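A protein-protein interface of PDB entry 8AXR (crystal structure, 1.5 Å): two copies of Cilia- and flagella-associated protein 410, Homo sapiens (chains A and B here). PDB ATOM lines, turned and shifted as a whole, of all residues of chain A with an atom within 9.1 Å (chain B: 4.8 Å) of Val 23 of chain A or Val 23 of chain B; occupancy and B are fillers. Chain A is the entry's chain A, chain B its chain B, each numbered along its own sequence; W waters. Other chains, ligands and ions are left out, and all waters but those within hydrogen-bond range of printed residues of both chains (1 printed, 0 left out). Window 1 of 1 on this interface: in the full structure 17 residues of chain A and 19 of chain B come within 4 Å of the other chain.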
ATOM      1  N   VAL A   4     -13.104  11.833  11.073  1.00  0.00           N
ATOM      2  CA  VAL A   4     -13.731  10.767  11.841  1.00  0.00           C
ATOM      3  C   VAL A   4     -15.077  10.411  11.229  1.00  0.00           C
ATOM      4  O   VAL A   4     -15.428   9.232  11.122  1.00  0.00           O
ATOM      5  CB  VAL A   4     -13.831  11.157  13.328  1.00  0.00           C
ATOM      6  CG1 VAL A   4     -14.677  10.162  14.085  1.00  0.00           C
ATOM      7  CG2 VAL A   4     -12.443  11.235  13.941  1.00  0.00           C
ATOM      8  N   LEU A   5     -15.832  11.421  10.775  1.00  0.00           N
ATOM      9  CA  LEU A   5     -17.108  11.141  10.121  1.00  0.00           C
ATOM     10  C   LEU A   5     -16.921  10.302   8.863  1.00  0.00           C
ATOM     11  O   LEU A   5     -17.680   9.355   8.629  1.00  0.00           O
ATOM     12  CB  LEU A   5     -17.852  12.435   9.798  1.00  0.00           C
ATOM     13  CG  LEU A   5     -19.172  12.272   9.033  1.00  0.00           C
ATOM     14  CD1 LEU A   5     -20.198  11.396   9.790  1.00  0.00           C
ATOM     15  CD2 LEU A   5     -19.762  13.644   8.715  1.00  0.00           C
ATOM     16  N   THR A   6     -15.926  10.638   8.031  1.00  0.00           N
ATOM     17  CA  THR A   6     -15.702   9.851   6.821  1.00  0.00           C
ATOM     18  C   THR A   6     -15.354   8.408   7.163  1.00  0.00           C
ATOM     19  O   THR A   6     -15.840   7.473   6.513  1.00  0.00           O
ATOM     20  CB  THR A   6     -14.599  10.483   5.967  1.00  0.00           C
ATOM     21  OG1 THR A   6     -15.008  11.788   5.544  1.00  0.00           O
ATOM     22  CG2 THR A   6     -14.313   9.635   4.726  1.00  0.00           C
ATOM     23  N   ALA A   7     -14.523   8.206   8.186  1.00  0.00           N
ATOM     24  CA  ALA A   7     -14.187   6.849   8.603  1.00  0.00           C
ATOM     25  C   ALA A   7     -15.418   6.097   9.091  1.00  0.00           C
ATOM     26  O   ALA A   7     -15.608   4.923   8.756  1.00  0.00           O
ATOM     27  CB  ALA A   7     -13.102   6.877   9.682  1.00  0.00           C
ATOM     28  N   ILE A   8     -16.274   6.757   9.877  1.00  0.00           N
ATOM     29  CA  ILE A   8     -17.471   6.077  10.365  1.00  0.00           C
ATOM     30  C   ILE A   8     -18.360   5.660   9.205  1.00  0.00           C
ATOM     31  O   ILE A   8     -18.887   4.540   9.179  1.00  0.00           O
ATOM     32  CB  ILE A   8     -18.242   6.953  11.369  1.00  0.00           C
ATOM     33  CG1 ILE A   8     -17.488   7.076  12.693  1.00  0.00           C
ATOM     34  CG2 ILE A   8     -19.635   6.363  11.626  1.00  0.00           C
ATOM     35  CD1 ILE A   8     -18.033   8.212  13.592  1.00  0.00           C
ATOM     36  N   LEU A   9     -18.566   6.558   8.238  1.00  0.00           N
ATOM     37  CA  LEU A   9     -19.488   6.249   7.151  1.00  0.00           C
ATOM     38  C   LEU A   9     -18.985   5.066   6.329  1.00  0.00           C
ATOM     39  O   LEU A   9     -19.781   4.229   5.876  1.00  0.00           O
ATOM     40  CB  LEU A   9     -19.713   7.480   6.274  1.00  0.00           C
ATOM     41  CG  LEU A   9     -20.384   8.688   6.934  1.00  0.00           C
ATOM     42  CD1 LEU A   9     -20.510   9.828   5.936  1.00  0.00           C
ATOM     43  CD2 LEU A   9     -21.730   8.321   7.501  1.00  0.00           C
ATOM     44  N   LEU A  10     -17.662   4.971   6.141  1.00  0.00           N
ATOM     45  CA  LEU A  10     -17.089   3.811   5.463  1.00  0.00           C
ATOM     46  C   LEU A  10     -17.308   2.537   6.272  1.00  0.00           C
ATOM     47  O   LEU A  10     -17.668   1.496   5.712  1.00  0.00           O
ATOM     48  CB  LEU A  10     -15.597   4.025   5.200  1.00  0.00           C
ATOM     49  CG  LEU A  10     -15.206   5.117   4.216  1.00  0.00           C
ATOM     50  CD1 LEU A  10     -13.720   5.370   4.332  1.00  0.00           C
ATOM     51  CD2 LEU A  10     -15.551   4.700   2.795  1.00  0.00           C
ATOM     52  N   LEU A  11     -17.115   2.601   7.594  1.00  0.00           N
ATOM     53  CA  LEU A  11     -17.264   1.399   8.411  1.00  0.00           C
ATOM     54  C   LEU A  11     -18.708   0.910   8.449  1.00  0.00           C
ATOM     55  O   LEU A  11     -18.946  -0.292   8.615  1.00  0.00           O
ATOM     56  CB  LEU A  11     -16.736   1.636   9.829  1.00  0.00           C
ATOM     57  CG  LEU A  11     -15.224   1.896   9.946  1.00  0.00           C
ATOM     58  CD1 LEU A  11     -14.909   2.440  11.333  1.00  0.00           C
ATOM     59  CD2 LEU A  11     -14.426   0.633   9.660  1.00  0.00           C
ATOM     60  N   LEU A  12     -19.675   1.817   8.277  1.00  0.00           N
ATOM     61  CA  LEU A  12     -21.082   1.419   8.266  1.00  0.00           C
ATOM     62  C   LEU A  12     -21.364   0.392   7.176  1.00  0.00           C
ATOM     63  O   LEU A  12     -22.259  -0.446   7.330  1.00  0.00           O
ATOM     64  CB  LEU A  12     -21.972   2.649   8.076  1.00  0.00           C
ATOM     65  CG  LEU A  12     -22.060   3.683   9.198  1.00  0.00           C
ATOM     66  CD1 LEU A  12     -22.965   4.835   8.763  1.00  0.00           C
ATOM     67  CD2 LEU A  12     -22.553   3.061  10.501  1.00  0.00           C
ATOM     68  N   LEU A  15     -21.263  -3.299   8.518  1.00  0.00           N
ATOM     69  CA  LEU A  15     -22.122  -3.746   9.606  1.00  0.00           C
ATOM     70  C   LEU A  15     -23.249  -4.636   9.100  1.00  0.00           C
ATOM     71  O   LEU A  15     -23.720  -4.499   7.968  1.00  0.00           O
ATOM     72  CB  LEU A  15     -22.751  -2.551  10.316  1.00  0.00           C
ATOM     73  CG  LEU A  15     -21.852  -1.641  11.142  1.00  0.00           C
ATOM     74  CD1 LEU A  15     -22.728  -0.653  11.891  1.00  0.00           C
ATOM     75  CD2 LEU A  15     -20.996  -2.459  12.093  1.00  0.00           C
ATOM     76  N   ASP A  16     -23.701  -5.535   9.970  1.00  0.00           N
ATOM     77  CA  ASP A  16     -24.895  -6.313   9.685  1.00  0.00           C
ATOM     78  C   ASP A  16     -26.117  -5.565  10.216  1.00  0.00           C
ATOM     79  O   ASP A  16     -26.006  -4.483  10.796  1.00  0.00           O
ATOM     80  CB  ASP A  16     -24.785  -7.739  10.240  1.00  0.00           C
ATOM     81  CG  ASP A  16     -24.533  -7.786  11.744  1.00  0.00           C
ATOM     82  OD1 ASP A  16     -24.551  -6.727  12.414  1.00  0.00           O
ATOM     83  OD2 ASP A  16     -24.309  -8.905  12.257  1.00  0.00           O
ATOM     84  N   ALA A  17     -27.302  -6.157  10.044  1.00  0.00           N
ATOM     85  CA  ALA A  17     -28.532  -5.482  10.447  1.00  0.00           C
ATOM     86  C   ALA A  17     -28.532  -5.145  11.934  1.00  0.00           C
ATOM     87  O   ALA A  17     -28.957  -4.051  12.330  1.00  0.00           O
ATOM     88  CB  ALA A  17     -29.733  -6.364  10.101  1.00  0.00           C
ATOM     89  N   GLU A  18     -28.065  -6.069  12.776  1.00  0.00           N
ATOM     90  CA  GLU A  18     -28.117  -5.840  14.216  1.00  0.00           C
ATOM     91  C   GLU A  18     -27.163  -4.716  14.607  1.00  0.00           C
ATOM     92  O   GLU A  18     -27.485  -3.889  15.465  1.00  0.00           O
ATOM     93  CB  GLU A  18     -27.752  -7.131  14.951  1.00  0.00           C
ATOM     94  CG  GLU A  18     -27.801  -7.102  16.494  1.00  0.00           C
ATOM     95  CD  GLU A  18     -28.914  -6.229  17.080  1.00  0.00           C
ATOM     96  OE1 GLU A  18     -28.677  -5.045  17.406  1.00  0.00           O
ATOM     97  OE2 GLU A  18     -30.050  -6.742  17.215  1.00  0.00           O
ATOM     98  N   GLY A  19     -25.992  -4.661  13.974  1.00  0.00           N
ATOM     99  CA  GLY A  19     -25.081  -3.559  14.233  1.00  0.00           C
ATOM    100  C   GLY A  19     -25.641  -2.224  13.784  1.00  0.00           C
ATOM    101  O   GLY A  19     -25.489  -1.212  14.478  1.00  0.00           O
ATOM    102  N   LEU A  20     -26.263  -2.188  12.600  1.00  0.00           N
ATOM    103  CA  LEU A  20     -26.888  -0.954  12.133  1.00  0.00           C
ATOM    104  C   LEU A  20     -27.967  -0.481  13.099  1.00  0.00           C
ATOM    105  O   LEU A  20     -28.091   0.722  13.356  1.00  0.00           O
ATOM    106  CB  LEU A  20     -27.478  -1.140  10.733  1.00  0.00           C
ATOM    107  CG  LEU A  20     -26.486  -1.315   9.580  1.00  0.00           C
ATOM    108  CD1 LEU A  20     -27.210  -1.750   8.318  1.00  0.00           C
ATOM    109  CD2 LEU A  20     -25.719  -0.016   9.343  1.00  0.00           C
ATOM    110  N   GLU A  21     -28.756  -1.411  13.648  1.00  0.00           N
ATOM    111  CA  GLU A  21     -29.803  -1.026  14.590  1.00  0.00           C
ATOM    112  C   GLU A  21     -29.218  -0.469  15.881  1.00  0.00           C
ATOM    113  O   GLU A  21     -29.798   0.442  16.486  1.00  0.00           O
ATOM    114  CB  GLU A  21     -30.695  -2.227  14.905  1.00  0.00           C
ATOM    115  CG  GLU A  21     -31.729  -2.533  13.838  1.00  0.00           C
ATOM    116  CD  GLU A  21     -32.471  -3.829  14.109  1.00  0.00           C
ATOM    117  OE1 GLU A  21     -32.965  -4.446  13.137  1.00  0.00           O
ATOM    118  OE2 GLU A  21     -32.552  -4.229  15.293  1.00  0.00           O
ATOM    119  N   ALA A  22     -28.086  -1.021  16.332  1.00  0.00           N
ATOM    120  CA  ALA A  22     -27.436  -0.497  17.531  1.00  0.00           C
ATOM    121  C   ALA A  22     -26.886   0.904  17.294  1.00  0.00           C
ATOM    122  O   ALA A  22     -26.968   1.758  18.184  1.00  0.00           O
ATOM    123  CB  ALA A  22     -26.341  -1.451  18.010  1.00  0.00           C
ATOM    124  N   VAL A  23     -26.332   1.166  16.105  1.00  0.00           N
ATOM    125  CA  VAL A  23     -25.872   2.521  15.792  1.00  0.00           C
ATOM    126  C   VAL A  23     -27.057   3.471  15.722  1.00  0.00           C
ATOM    127  O   VAL A  23     -27.010   4.587  16.251  1.00  0.00           O
ATOM    128  CB  VAL A  23     -25.058   2.537  14.482  1.00  0.00           C
ATOM    129  CG1 VAL A  23     -24.712   3.991  14.082  1.00  0.00           C
ATOM    130  CG2 VAL A  23     -23.783   1.707  14.621  1.00  0.00           C
ATOM    131  N   GLN A  24     -28.142   3.034  15.078  1.00  0.00           N
ATOM    132  CA  GLN A  24     -29.349   3.848  14.981  1.00  0.00           C
ATOM    133  C   GLN A  24     -29.844   4.249  16.363  1.00  0.00           C
ATOM    134  O   GLN A  24     -30.199   5.411  16.602  1.00  0.00           O
ATOM    135  CB  GLN A  24     -30.437   3.050  14.262  1.00  0.00           C
ATOM    136  CG  GLN A  24     -31.590   3.905  13.761  1.00  0.00           C
ATOM    137  CD  GLN A  24     -32.595   3.098  12.971  1.00  0.00           C
ATOM    138  OE1 GLN A  24     -33.117   2.088  13.455  1.00  0.00           O
ATOM    139  NE2 GLN A  24     -32.853   3.519  11.737  1.00  0.00           N
ATOM    140  N   GLN A  25     -29.879   3.295  17.295  1.00  0.00           N
ATOM    141  CA  GLN A  25     -30.406   3.587  18.625  1.00  0.00           C
ATOM    142  C   GLN A  25     -29.472   4.512  19.402  1.00  0.00           C
ATOM    143  O   GLN A  25     -29.932   5.416  20.113  1.00  0.00           O
ATOM    144  CB  GLN A  25     -30.639   2.276  19.372  1.00  0.00           C
ATOM    145  CG  GLN A  25     -30.847   2.400  20.871  1.00  0.00           C
ATOM    146  CD  GLN A  25     -30.713   1.059  21.573  1.00  0.00           C
ATOM    147  OE1 GLN A  25     -31.707   0.459  21.979  1.00  0.00           O
ATOM    148  NE2 GLN A  25     -29.476   0.588  21.725  1.00  0.00           N
ATOM    149  N   THR A  26     -28.159   4.326  19.250  1.00  0.00           N
ATOM    150  CA  THR A  26     -27.192   5.153  19.967  1.00  0.00           C
ATOM    151  C   THR A  26     -27.210   6.585  19.452  1.00  0.00           C
ATOM    152  O   THR A  26     -27.217   7.542  20.237  1.00  0.00           O
ATOM    153  CB  THR A  26     -25.797   4.545  19.819  1.00  0.00           C
ATOM    154  OG1 THR A  26     -25.794   3.212  20.353  1.00  0.00           O
ATOM    155  CG2 THR A  26     -24.746   5.403  20.534  1.00  0.00           C
ATOM    156  N   VAL A  27     -27.192   6.755  18.129  1.00  0.00           N
ATOM    157  CA  VAL A  27     -27.198   8.099  17.554  1.00  0.00           C
ATOM    158  C   VAL A  27     -28.495   8.818  17.906  1.00  0.00           C
ATOM    159  O   VAL A  27     -28.495  10.013  18.240  1.00  0.00           O
ATOM    160  CB  VAL A  27     -26.963   8.026  16.034  1.00  0.00           C
ATOM    161  CG1 VAL A  27     -27.318   9.344  15.363  1.00  0.00           C
ATOM    162  CG2 VAL A  27     -25.518   7.632  15.728  1.00  0.00           C
ATOM    163  N   GLY A  28     -29.619   8.103  17.853  1.00  0.00           N
ATOM    164  CA  GLY A  28     -30.888   8.719  18.205  1.00  0.00           C
ATOM    165  C   GLY A  28     -30.918   9.204  19.641  1.00  0.00           C
ATOM    166  O   GLY A  28     -31.469  10.267  19.937  1.00  0.00           O
ATOM    167  N   SER A  29     -30.306   8.444  20.550  1.00  0.00           N
ATOM    168  CA  SER A  29     -30.242   8.868  21.944  1.00  0.00           C
ATOM    169  C   SER A  29     -29.327  10.080  22.115  1.00  0.00           C
ATOM    170  O   SER A  29     -29.595  10.956  22.948  1.00  0.00           O
ATOM    171  CB  SER A  29     -29.792   7.698  22.822  1.00  0.00           C
ATOM    172  OG  SER A  29     -29.407   8.143  24.110  1.00  0.00           O
ATOM    173  N   ARG A  30     -28.247  10.154  21.333  1.00  0.00           N
ATOM    174  CA  ARG A  30     -27.371  11.321  21.400  1.00  0.00           C
ATOM    175  C   ARG A  30     -28.052  12.553  20.815  1.00  0.00           C
ATOM    176  O   ARG A  30     -27.894  13.664  21.337  1.00  0.00           O
ATOM    177  CB  ARG A  30     -26.072  11.046  20.642  1.00  0.00           C
ATOM    178  CG  ARG A  30     -25.013  10.284  21.423  1.00  0.00           C
ATOM    179  CD  ARG A  30     -23.989  11.202  22.103  1.00  0.00           C
ATOM    180  NE  ARG A  30     -23.670  12.415  21.357  1.00  0.00           N
ATOM    181  CZ  ARG A  30     -22.511  12.642  20.748  1.00  0.00           C
ATOM    182  NH1 ARG A  30     -21.594  11.694  20.635  1.00  0.00           N
ATOM    183  NH2 ARG A  30     -22.272  13.844  20.227  1.00  0.00           N
ATOM    184  N   LEU A  31     -28.800  12.377  19.722  1.00  0.00           N
ATOM    185  CA  LEU A  31     -29.447  13.508  19.063  1.00  0.00           C
ATOM    186  C   LEU A  31     -30.615  14.050  19.877  1.00  0.00           C
ATOM    187  O   LEU A  31     -30.837  15.264  19.908  1.00  0.00           O
ATOM    188  CB  LEU A  31     -29.911  13.108  17.661  1.00  0.00           C
ATOM    189  CG  LEU A  31     -28.825  13.068  16.580  1.00  0.00           C
ATOM    190  CD1 LEU A  31     -29.316  12.334  15.343  1.00  0.00           C
ATOM    191  CD2 LEU A  31     -28.427  14.497  16.229  1.00  0.00           C
ATOM    192  N   LEU B   5     -18.478  -2.647  15.035  1.00  0.00           N
ATOM    193  CA  LEU B   5     -19.526  -1.950  15.778  1.00  0.00           C
ATOM    194  C   LEU B   5     -18.946  -1.196  16.971  1.00  0.00           C
ATOM    195  O   LEU B   5     -19.237  -0.008  17.179  1.00  0.00           O
ATOM    196  CB  LEU B   5     -20.597  -2.948  16.232  1.00  0.00           C
ATOM    197  CG  LEU B   5     -21.714  -2.364  17.097  1.00  0.00           C
ATOM    198  CD1 LEU B   5     -22.395  -1.194  16.397  1.00  0.00           C
ATOM    199  CD2 LEU B   5     -22.743  -3.430  17.490  1.00  0.00           C
ATOM    200  N   ILE B   8     -17.066   1.902  15.856  1.00  0.00           N
ATOM    201  CA  ILE B   8     -17.989   2.963  15.452  1.00  0.00           C
ATOM    202  C   ILE B   8     -18.584   3.653  16.675  1.00  0.00           C
ATOM    203  O   ILE B   8     -18.630   4.885  16.750  1.00  0.00           O
ATOM    204  CB  ILE B   8     -19.093   2.413  14.529  1.00  0.00           C
ATOM    205  CG1 ILE B   8     -18.522   2.007  13.163  1.00  0.00           C
ATOM    206  CG2 ILE B   8     -20.206   3.451  14.342  1.00  0.00           C
ATOM    207  CD1 ILE B   8     -19.510   1.159  12.352  1.00  0.00           C
ATOM    208  N   LEU B   9     -19.064   2.868  17.644  1.00  0.00           N
ATOM    209  CA  LEU B   9     -19.714   3.463  18.810  1.00  0.00           C
ATOM    210  C   LEU B   9     -18.731   4.293  19.627  1.00  0.00           C
ATOM    211  O   LEU B   9     -19.089   5.350  20.164  1.00  0.00           O
ATOM    212  CB  LEU B   9     -20.339   2.356  19.661  1.00  0.00           C
ATOM    213  CG  LEU B   9     -21.567   1.667  19.053  1.00  0.00           C
ATOM    214  CD1 LEU B   9     -22.298   0.893  20.137  1.00  0.00           C
ATOM    215  CD2 LEU B   9     -22.527   2.642  18.381  1.00  0.00           C
ATOM    216  N   LEU B  12     -18.224   7.683  17.822  1.00  0.00           N
ATOM    217  CA  LEU B  12     -19.354   8.603  17.746  1.00  0.00           C
ATOM    218  C   LEU B  12     -19.186   9.815  18.654  1.00  0.00           C
ATOM    219  O   LEU B  12     -19.764  10.869  18.388  1.00  0.00           O
ATOM    220  CB  LEU B  12     -20.656   7.883  18.111  1.00  0.00           C
ATOM    221  CG  LEU B  12     -21.223   6.907  17.087  1.00  0.00           C
ATOM    222  CD1 LEU B  12     -22.515   6.311  17.649  1.00  0.00           C
ATOM    223  CD2 LEU B  12     -21.494   7.616  15.779  1.00  0.00           C
ATOM    224  N   LEU B  15     -18.036  13.143  17.309  1.00  0.00           N
ATOM    225  CA  LEU B  15     -18.948  13.845  16.419  1.00  0.00           C
ATOM    226  C   LEU B  15     -19.811  14.828  17.196  1.00  0.00           C
ATOM    227  O   LEU B  15     -20.106  14.629  18.379  1.00  0.00           O
ATOM    228  CB  LEU B  15     -19.876  12.863  15.701  1.00  0.00           C
ATOM    229  CG  LEU B  15     -19.264  11.894  14.694  1.00  0.00           C
ATOM    230  CD1 LEU B  15     -20.382  11.130  13.974  1.00  0.00           C
ATOM    231  CD2 LEU B  15     -18.383  12.642  13.705  1.00  0.00           C
ATOM    232  N   GLY B  19     -22.618  15.783  12.439  1.00  0.00           N
ATOM    233  CA  GLY B  19     -22.080  14.486  12.057  1.00  0.00           C
ATOM    234  C   GLY B  19     -22.981  13.342  12.480  1.00  0.00           C
ATOM    235  O   GLY B  19     -23.107  12.340  11.766  1.00  0.00           O
ATOM    236  N   LEU B  20     -23.614  13.468  13.647  1.00  0.00           N
ATOM    237  CA  LEU B  20     -24.543  12.432  14.089  1.00  0.00           C
ATOM    238  C   LEU B  20     -25.732  12.323  13.142  1.00  0.00           C
ATOM    239  O   LEU B  20     -26.193  11.215  12.841  1.00  0.00           O
ATOM    240  CB  LEU B  20     -25.008  12.729  15.515  1.00  0.00           C
ATOM    241  CG  LEU B  20     -23.976  12.557  16.630  1.00  0.00           C
ATOM    242  CD1 LEU B  20     -24.495  13.195  17.912  1.00  0.00           C
ATOM    243  CD2 LEU B  20     -23.638  11.093  16.855  1.00  0.00           C
ATOM    244  N   GLU B  21     -26.250  13.460  12.665  1.00  0.00           N
ATOM    245  CA  GLU B  21     -27.353  13.423  11.708  1.00  0.00           C
ATOM    246  C   GLU B  21     -26.937  12.742  10.411  1.00  0.00           C
ATOM    247  O   GLU B  21     -27.729  12.010   9.802  1.00  0.00           O
ATOM    248  CB  GLU B  21     -27.857  14.837  11.425  1.00  0.00           C
ATOM    249  CG  GLU B  21     -28.835  15.365  12.459  1.00  0.00           C
ATOM    250  CD  GLU B  21     -28.686  16.859  12.677  1.00  0.00           C
ATOM    251  OE1 GLU B  21     -28.475  17.285  13.836  1.00  0.00           O
ATOM    252  OE2 GLU B  21     -28.773  17.605  11.677  1.00  0.00           O
ATOM    253  N   ALA B  22     -25.701  12.981   9.963  1.00  0.00           N
ATOM    254  CA  ALA B  22     -25.197  12.298   8.776  1.00  0.00           C
ATOM    255  C   ALA B  22     -25.175  10.788   8.986  1.00  0.00           C
ATOM    256  O   ALA B  22     -25.601  10.019   8.116  1.00  0.00           O
ATOM    257  CB  ALA B  22     -23.808  12.834   8.420  1.00  0.00           C
ATOM    258  N   VAL B  23     -24.681  10.346  10.145  1.00  0.00           N
ATOM    259  CA  VAL B  23     -24.660   8.918  10.454  1.00  0.00           C
ATOM    260  C   VAL B  23     -26.075   8.355  10.472  1.00  0.00           C
ATOM    261  O   VAL B  23     -26.351   7.306   9.880  1.00  0.00           O
ATOM    262  CB  VAL B  23     -23.928   8.667  11.783  1.00  0.00           C
ATOM    263  CG1 VAL B  23     -24.113   7.213  12.240  1.00  0.00           C
ATOM    264  CG2 VAL B  23     -22.443   9.048  11.639  1.00  0.00           C
ATOM    265  N   GLN B  24     -26.998   9.053  11.142  1.00  0.00           N
ATOM    266  CA  GLN B  24     -28.356   8.535  11.277  1.00  0.00           C
ATOM    267  C   GLN B  24     -29.025   8.382   9.915  1.00  0.00           C
ATOM    268  O   GLN B  24     -29.735   7.397   9.667  1.00  0.00           O
ATOM    269  CB  GLN B  24     -29.184   9.453  12.180  1.00  0.00           C
ATOM    270  CG  GLN B  24     -30.552   8.880  12.576  1.00  0.00           C
ATOM    271  CD  GLN B  24     -30.443   7.598  13.405  1.00  0.00           C
ATOM    272  OE1 GLN B  24     -29.988   6.556  12.924  1.00  0.00           O
ATOM    273  NE2 GLN B  24     -30.869   7.675  14.663  1.00  0.00           N
ATOM    274  N   GLN B  25     -28.795   9.339   9.013  1.00  0.00           N
ATOM    275  CA  GLN B  25     -29.409   9.277   7.690  1.00  0.00           C
ATOM    276  C   GLN B  25     -28.831   8.130   6.866  1.00  0.00           C
ATOM    277  O   GLN B  25     -29.575   7.414   6.183  1.00  0.00           O
ATOM    278  CB  GLN B  25     -29.238  10.619   6.977  1.00  0.00           C
ATOM    279  CG  GLN B  25     -30.524  11.153   6.362  1.00  0.00           C
ATOM    280  CD  GLN B  25     -30.276  12.183   5.277  1.00  0.00           C
ATOM    281  OE1 GLN B  25     -29.175  12.722   5.155  1.00  0.00           O
ATOM    282  NE2 GLN B  25     -31.301  12.461   4.479  1.00  0.00           N
ATOM    283  N   THR B  26     -27.509   7.935   6.924  1.00  0.00           N
ATOM    284  CA  THR B  26     -26.892   6.804   6.234  1.00  0.00           C
ATOM    285  C   THR B  26     -27.395   5.475   6.787  1.00  0.00           C
ATOM    286  O   THR B  26     -27.689   4.548   6.025  1.00  0.00           O
ATOM    287  CB  THR B  26     -25.368   6.892   6.349  1.00  0.00           C
ATOM    288  OG1 THR B  26     -24.915   8.128   5.783  1.00  0.00           O
ATOM    289  CG2 THR B  26     -24.707   5.734   5.622  1.00  0.00           C
ATOM    290  N   VAL B  27     -27.505   5.368   8.115  1.00  0.00           N
ATOM    291  CA  VAL B  27     -27.960   4.125   8.733  1.00  0.00           C
ATOM    292  C   VAL B  27     -29.406   3.831   8.348  1.00  0.00           C
ATOM    293  O   VAL B  27     -29.760   2.689   8.029  1.00  0.00           O
ATOM    294  CB  VAL B  27     -27.770   4.191  10.261  1.00  0.00           C
ATOM    295  CG1 VAL B  27     -28.589   3.125  10.947  1.00  0.00           C
ATOM    296  CG2 VAL B  27     -26.294   4.049  10.631  1.00  0.00           C
HETATM  297  O   HOH W   1     -31.907   5.845  11.020  1.00  0.00           O
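The backbone carbonyl oxygen of Gln 24 of chain A is in hydrogen-bond range of the side-chain amide nitrogen of Gln 24 of chain B (3.1 Å). NE2 of Gln 24 of chain B sits close to N of Gly 28 of chain A. The guanidinium group (NH1) of Arg 30 of chain A lies within hydrogen-bond range of the backbone carbonyl oxygen (O) of Leu 12 of chain B. The backbone carbonyl oxygen (O) of Leu 15 of chain B lies within hydrogen-bond range of the guanidinium group (NH2) of Arg 30 of chain A (3.0 Å).
The side-chain carboxylate (OD1) of Asp 16 of chain A is in hydrogen-bond range of the backbone NH (N) of Gly 19 of chain A (3.0 Å). O of Ala 22 of chain A is in hydrogen-bond range of OG1 of Thr 26 of chain A (2.9 Å). The side-chain hydroxyl (OG1) of Thr 26 of chain B lies within hydrogen-bond range of the backbone carbonyl oxygen (O) of Ala 22 of chain B (3.1 Å).
CD2 of Leu 15 of chain B touches CB of Leu 5 of chain A, at 3.9 Å. CG2 of Thr 26 of chain B touches CD1 of Leu 12 of chain A, at 3.7 Å. Val 27 of chain B touches Leu 12 of chain A. Ile 8 of chain B touches Leu 15 of chain A (CD1 to CD1, 3.7 Å). Gly 19 of chain A touches Leu 5 of chain B (O to CD1, 3.6 Å). CG1 of Val 27 of chain B touches O of Leu 20 of chain A, at 3.4 Å. CG2 of Val 23 of chain A touches CD1 of Leu 5 of chain B (3.7 Å). Val 27 of chain B touches Val 23 of chain A (CG2 to CG1, 3.8 Å). CD1 of Leu 12 of chain B touches CG2 of Thr 26 of chain A (3.8 Å). Leu 31 of chain A touches Glu 21 of chain B.
Of the printed residues of chain B, Gly 19 of chain A touches Leu 5. Printed residues of chain B within 4 Å of Val 27 of chain A: Leu 12 (3.8 Å), Leu 20 (3.3 Å), Val 23 (3.8 Å) and Gln 24 (3.7 Å). Of the printed residues of chain B, Gly 28 of chain A touches Gln 24. Of the printed residues of chain A, Leu 15 of chain B touches Leu 5 (3.9 Å), Ile 8 (3.8 Å) and Arg 30 (3.0 Å). No residue of chain A comes within 4 Å of Ala 22 of chain B. Of chain A, only Leu 5, Ile 8, Val 23 and Val 27 come within 4 Å of Val 23 of chain B. Of chain A, only Leu 9 and Leu 12 come within 4 Å of Thr 26 of chain B. Of the printed residues of chain A, Val 27 of chain B touches Leu 12 (3.9 Å), Leu 20 (3.4 Å), Val 23 (3.8 Å) and Gln 24 (3.8 Å). The nearest printed residue of chain B that does not touch Val 23 of chain A is Leu 9 of chain B (4.1 Å).
Of the 26 printed residues of chain A, 15 touch a printed residue of chain B. Printed residues of chain A that touch a printed residue of chain B: Leu 5, Ile 8, Leu 9, Leu 11, Leu 12, Leu 15, Gly 19, Leu 20, Val 23, Gln 24, Thr 26, Val 27, Gly 28, Arg 30 and Leu 31. Hydrophobic or aromatic side chains of chain A within 4 Å of the printed part of chain B: Leu 5, Ile 8, Leu 9, Leu 11, Leu 12, Leu 15, Val 23, Val 27 and Leu 31. Along chain A the printed residues that touch a printed residue of chain B span positions 5 to 31. Among the printed residues, no Asp or Glu carboxylate lies within 4 Å of a Lys or Arg side-chain nitrogen of the other chain.
Leu 5 of chain A touches Val 23 of chain B, and with the chains exchanged Val 23 of chain A touches Leu 5 of chain B. Ile 8 of chain A touches Val 23 of chain B, and with the chains exchanged Val 23 of chain A touches Ile 8 of chain B. Leu 12 of chain A touches Val 27 of chain B, and with the chains exchanged Val 27 of chain A touches Leu 12 of chain B. Val 23 of chain A touches its own counterpart, Val 23 of chain B. 14 positions are printed for both chains.
Water W1 bridges the side-chain amide nitrogen (NE2) of Gln 24 of chain A and the side-chain amide oxygen (OE1) of Gln 24 of chain B.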
